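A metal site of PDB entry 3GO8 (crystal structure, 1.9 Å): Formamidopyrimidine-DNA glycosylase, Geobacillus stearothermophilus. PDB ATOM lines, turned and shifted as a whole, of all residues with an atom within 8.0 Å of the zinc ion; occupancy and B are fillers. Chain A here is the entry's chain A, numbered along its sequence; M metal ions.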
ATOM      1  N   PHE A 181      31.635   8.507 -10.551  1.00  0.00           N
ATOM      2  CA  PHE A 181      30.480   7.613 -10.365  1.00  0.00           C
ATOM      3  C   PHE A 181      30.464   6.504 -11.426  1.00  0.00           C
ATOM      4  O   PHE A 181      30.358   5.316 -11.103  1.00  0.00           O
ATOM      5  CB  PHE A 181      29.144   8.382 -10.406  1.00  0.00           C
ATOM      6  CG  PHE A 181      27.955   7.467 -10.463  1.00  0.00           C
ATOM      7  CD1 PHE A 181      27.484   6.868  -9.300  1.00  0.00           C
ATOM      8  CD2 PHE A 181      27.363   7.139 -11.688  1.00  0.00           C
ATOM      9  CE1 PHE A 181      26.421   6.000  -9.349  1.00  0.00           C
ATOM     10  CE2 PHE A 181      26.290   6.257 -11.721  1.00  0.00           C
ATOM     11  CZ  PHE A 181      25.815   5.701 -10.563  1.00  0.00           C
ATOM     12  N   TYR A 223      23.864  11.375 -13.130  1.00  0.00           N
ATOM     13  CA  TYR A 223      23.699  10.306 -12.145  1.00  0.00           C
ATOM     14  C   TYR A 223      23.780  10.785 -10.710  1.00  0.00           C
ATOM     15  O   TYR A 223      23.080  10.259  -9.831  1.00  0.00           O
ATOM     16  CB  TYR A 223      24.739   9.226 -12.352  1.00  0.00           C
ATOM     17  CG  TYR A 223      24.525   8.418 -13.613  1.00  0.00           C
ATOM     18  CD1 TYR A 223      25.338   8.602 -14.727  1.00  0.00           C
ATOM     19  CD2 TYR A 223      23.492   7.474 -13.694  1.00  0.00           C
ATOM     20  CE1 TYR A 223      25.150   7.865 -15.890  1.00  0.00           C
ATOM     21  CE2 TYR A 223      23.286   6.735 -14.844  1.00  0.00           C
ATOM     22  CZ  TYR A 223      24.117   6.937 -15.945  1.00  0.00           C
ATOM     23  OH  TYR A 223      23.925   6.208 -17.097  1.00  0.00           O
ATOM     24  N   VAL A 224      24.652  11.769 -10.466  1.00  0.00           N
ATOM     25  CA  VAL A 224      24.943  12.196  -9.098  1.00  0.00           C
ATOM     26  C   VAL A 224      24.970  13.701  -8.870  1.00  0.00           C
ATOM     27  O   VAL A 224      24.599  14.160  -7.792  1.00  0.00           O
ATOM     28  CB  VAL A 224      26.264  11.556  -8.543  1.00  0.00           C
ATOM     29  CG1 VAL A 224      26.144  10.036  -8.490  1.00  0.00           C
ATOM     30  CG2 VAL A 224      27.500  11.973  -9.345  1.00  0.00           C
ATOM     31  N   PRO A 231      17.393   9.051  -5.033  1.00  0.00           N
ATOM     32  CA  PRO A 231      17.903   7.702  -5.272  1.00  0.00           C
ATOM     33  C   PRO A 231      18.913   7.636  -6.431  1.00  0.00           C
ATOM     34  O   PRO A 231      18.698   8.257  -7.493  1.00  0.00           O
ATOM     35  CB  PRO A 231      16.649   6.902  -5.632  1.00  0.00           C
ATOM     36  CG  PRO A 231      15.513   7.705  -5.115  1.00  0.00           C
ATOM     37  CD  PRO A 231      15.937   9.124  -5.252  1.00  0.00           C
ATOM     38  N   CYS A 232      19.998   6.895  -6.211  1.00  0.00           N
ATOM     39  CA  CYS A 232      20.913   6.527  -7.285  1.00  0.00           C
ATOM     40  C   CYS A 232      20.113   5.876  -8.408  1.00  0.00           C
ATOM     41  O   CYS A 232      19.226   5.025  -8.160  1.00  0.00           O
ATOM     42  CB  CYS A 232      21.962   5.539  -6.751  1.00  0.00           C
ATOM     43  SG  CYS A 232      23.136   4.933  -8.030  1.00  0.00           S
ATOM     44  N   LYS A 233      20.412   6.267  -9.638  1.00  0.00           N
ATOM     45  CA  LYS A 233      19.718   5.726 -10.809  1.00  0.00           C
ATOM     46  C   LYS A 233      20.116   4.275 -11.141  1.00  0.00           C
ATOM     47  O   LYS A 233      19.450   3.605 -11.940  1.00  0.00           O
ATOM     48  CB  LYS A 233      19.966   6.618 -12.038  1.00  0.00           C
ATOM     49  CG  LYS A 233      19.419   8.023 -11.867  1.00  0.00           C
ATOM     50  CD  LYS A 233      19.586   8.843 -13.132  1.00  0.00           C
ATOM     51  CE  LYS A 233      18.809  10.149 -13.003  1.00  0.00           C
ATOM     52  NZ  LYS A 233      19.101  11.090 -14.129  1.00  0.00           N
ATOM     53  N   ARG A 234      21.207   3.813 -10.538  1.00  0.00           N
ATOM     54  CA  ARG A 234      21.730   2.460 -10.759  1.00  0.00           C
ATOM     55  C   ARG A 234      21.252   1.499  -9.670  1.00  0.00           C
ATOM     56  O   ARG A 234      20.887   0.362  -9.966  1.00  0.00           O
ATOM     57  CB  ARG A 234      23.273   2.490 -10.853  1.00  0.00           C
ATOM     58  CG  ARG A 234      23.953   1.127 -10.943  1.00  0.00           C
ATOM     59  CD  ARG A 234      25.156   1.126 -11.891  1.00  0.00           C
ATOM     60  NE  ARG A 234      26.320   1.869 -11.394  1.00  0.00           N
ATOM     61  CZ  ARG A 234      27.305   2.326 -12.164  1.00  0.00           C
ATOM     62  NH1 ARG A 234      27.269   2.139 -13.483  1.00  0.00           N
ATOM     63  NH2 ARG A 234      28.333   2.995 -11.641  1.00  0.00           N
ATOM     64  N   CYS A 235      21.256   1.946  -8.422  1.00  0.00           N
ATOM     65  CA  CYS A 235      20.992   1.040  -7.274  1.00  0.00           C
ATOM     66  C   CYS A 235      19.938   1.498  -6.282  1.00  0.00           C
ATOM     67  O   CYS A 235      19.581   0.736  -5.377  1.00  0.00           O
ATOM     68  CB  CYS A 235      22.293   0.745  -6.512  1.00  0.00           C
ATOM     69  SG  CYS A 235      22.840   2.131  -5.464  1.00  0.00           S
ATOM     70  N   GLY A 236      19.471   2.739  -6.412  1.00  0.00           N
ATOM     71  CA  GLY A 236      18.431   3.263  -5.538  1.00  0.00           C
ATOM     72  C   GLY A 236      18.895   3.803  -4.192  1.00  0.00           C
ATOM     73  O   GLY A 236      18.094   4.386  -3.477  1.00  0.00           O
ATOM     74  N   THR A 237      20.171   3.626  -3.849  1.00  0.00           N
ATOM     75  CA  THR A 237      20.742   4.227  -2.606  1.00  0.00           C
ATOM     76  C   THR A 237      20.753   5.763  -2.728  1.00  0.00           C
ATOM     77  O   THR A 237      21.067   6.282  -3.785  1.00  0.00           O
ATOM     78  CB  THR A 237      22.200   3.730  -2.364  1.00  0.00           C
ATOM     79  OG1 THR A 237      22.192   2.301  -2.220  1.00  0.00           O
ATOM     80  CG2 THR A 237      22.836   4.361  -1.127  1.00  0.00           C
ATOM     81  N   PRO A 238      20.352   6.490  -1.660  1.00  0.00           N
ATOM     82  CA  PRO A 238      20.417   7.944  -1.733  1.00  0.00           C
ATOM     83  C   PRO A 238      21.817   8.461  -2.042  1.00  0.00           C
ATOM     84  O   PRO A 238      22.823   8.037  -1.421  1.00  0.00           O
ATOM     85  CB  PRO A 238      19.943   8.393  -0.354  1.00  0.00           C
ATOM     86  CG  PRO A 238      19.087   7.257   0.134  1.00  0.00           C
ATOM     87  CD  PRO A 238      19.787   6.030  -0.370  1.00  0.00           C
ATOM     88  N   ILE A 239      21.884   9.364  -3.010  1.00  0.00           N
ATOM     89  CA  ILE A 239      23.126  10.014  -3.357  1.00  0.00           C
ATOM     90  C   ILE A 239      23.546  10.908  -2.186  1.00  0.00           C
ATOM     91  O   ILE A 239      22.694  11.526  -1.538  1.00  0.00           O
ATOM     92  CB  ILE A 239      22.981  10.812  -4.682  1.00  0.00           C
ATOM     93  CG1 ILE A 239      22.666   9.850  -5.831  1.00  0.00           C
ATOM     94  CG2 ILE A 239      24.223  11.685  -4.974  1.00  0.00           C
ATOM     95  CD1 ILE A 239      23.651   8.653  -5.964  1.00  0.00           C
ATOM     96  N   TYR A 251      28.136  11.601  -4.782  1.00  0.00           N
ATOM     97  CA  TYR A 251      28.560  10.227  -4.992  1.00  0.00           C
ATOM     98  C   TYR A 251      27.523   9.231  -4.473  1.00  0.00           C
ATOM     99  O   TYR A 251      26.710   9.563  -3.581  1.00  0.00           O
ATOM    100  CB  TYR A 251      29.936   9.955  -4.346  1.00  0.00           C
ATOM    101  CG  TYR A 251      29.929  10.062  -2.835  1.00  0.00           C
ATOM    102  CD1 TYR A 251      29.745   8.932  -2.046  1.00  0.00           C
ATOM    103  CD2 TYR A 251      30.081  11.295  -2.197  1.00  0.00           C
ATOM    104  CE1 TYR A 251      29.696   9.014  -0.655  1.00  0.00           C
ATOM    105  CE2 TYR A 251      30.041  11.395  -0.798  1.00  0.00           C
ATOM    106  CZ  TYR A 251      29.849  10.242  -0.041  1.00  0.00           C
ATOM    107  OH  TYR A 251      29.821  10.294   1.344  1.00  0.00           O
ATOM    108  N   CYS A 252      27.540   8.029  -5.035  1.00  0.00           N
ATOM    109  CA  CYS A 252      26.755   6.923  -4.502  1.00  0.00           C
ATOM    110  C   CYS A 252      27.659   6.123  -3.582  1.00  0.00           C
ATOM    111  O   CYS A 252      28.673   5.572  -4.024  1.00  0.00           O
ATOM    112  CB  CYS A 252      26.230   6.017  -5.605  1.00  0.00           C
ATOM    113  SG  CYS A 252      25.379   4.604  -4.914  1.00  0.00           S
ATOM    114  N   PRO A 253      27.313   6.067  -2.289  1.00  0.00           N
ATOM    115  CA  PRO A 253      28.179   5.349  -1.363  1.00  0.00           C
ATOM    116  C   PRO A 253      28.172   3.820  -1.527  1.00  0.00           C
ATOM    117  O   PRO A 253      29.040   3.155  -0.960  1.00  0.00           O
ATOM    118  CB  PRO A 253      27.596   5.720   0.010  1.00  0.00           C
ATOM    119  CG  PRO A 253      26.168   5.973  -0.240  1.00  0.00           C
ATOM    120  CD  PRO A 253      26.118   6.634  -1.608  1.00  0.00           C
ATOM    121  N   ARG A 254      27.207   3.263  -2.249  1.00  0.00           N
ATOM    122  CA  ARG A 254      27.228   1.829  -2.529  1.00  0.00           C
ATOM    123  C   ARG A 254      28.081   1.495  -3.758  1.00  0.00           C
ATOM    124  O   ARG A 254      28.912   0.593  -3.721  1.00  0.00           O
ATOM    125  CB  ARG A 254      25.801   1.302  -2.711  1.00  0.00           C
ATOM    126  CG  ARG A 254      25.742  -0.141  -3.188  1.00  0.00           C
ATOM    127  CD  ARG A 254      24.324  -0.654  -3.340  1.00  0.00           C
ATOM    128  NE  ARG A 254      24.358  -2.056  -3.723  1.00  0.00           N
ATOM    129  CZ  ARG A 254      23.311  -2.856  -3.808  1.00  0.00           C
ATOM    130  NH1 ARG A 254      23.508  -4.138  -4.147  1.00  0.00           N
ATOM    131  NH2 ARG A 254      22.074  -2.414  -3.510  1.00  0.00           N
ATOM    132  N   CYS A 255      27.878   2.242  -4.835  1.00  0.00           N
ATOM    133  CA  CYS A 255      28.477   1.880  -6.106  1.00  0.00           C
ATOM    134  C   CYS A 255      29.920   2.337  -6.276  1.00  0.00           C
ATOM    135  O   CYS A 255      30.673   1.723  -7.035  1.00  0.00           O
ATOM    136  CB  CYS A 255      27.603   2.386  -7.240  1.00  0.00           C
ATOM    137  SG  CYS A 255      25.973   1.572  -7.150  1.00  0.00           S
ATOM    138  N   GLN A 256      30.298   3.384  -5.550  1.00  0.00           N
ATOM    139  CA  GLN A 256      31.655   3.891  -5.607  1.00  0.00           C
ATOM    140  C   GLN A 256      32.501   3.379  -4.443  1.00  0.00           C
ATOM    141  O   GLN A 256      32.035   3.367  -3.300  1.00  0.00           O
ATOM    142  CB  GLN A 256      31.627   5.414  -5.660  1.00  0.00           C
ATOM    143  CG  GLN A 256      31.039   5.901  -6.977  1.00  0.00           C
ATOM    144  CD  GLN A 256      30.740   7.388  -6.977  1.00  0.00           C
ATOM    145  OE1 GLN A 256      29.590   7.796  -6.917  1.00  0.00           O
ATOM    146  NE2 GLN A 256      31.779   8.204  -7.068  1.00  0.00           N
HETATM  147 ZN    ZN M   1      24.240   3.548  -6.616  1.00  0.00          ZN
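The side-chain sulfur of Cys 235 lies close to the side-chain hydroxyl of Thr 237, 3.3 Å away. The backbone NH of Cys 252 lies within hydrogen-bond range of the side-chain amide oxygen of Gln 256 (2.8 Å). SG of Cys 232 sits close to N of Arg 234 (3.4 Å). N of Cys 232 sits at hydrogen-bond distance from O of Thr 237. SG of Cys 252 lies close to N of Arg 254, 3.5 Å away.
Within 4 Å of the zinc ion: Cys 232, Cys 235, Cys 252 and Cys 255. Along chain A the residues within 4 Å of the zinc ion span positions 232 to 255.
SG of Cys 232 is bound to the zinc ion. SG of Cys 235 is bound to the zinc ion, at 2.3 Å. SG of Cys 252 is bound to the zinc ion, at 2.3 Å. The zinc ion is bound by SG of Cys 255 (2.7 Å). The zinc ion has four donor atoms within binding distance.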
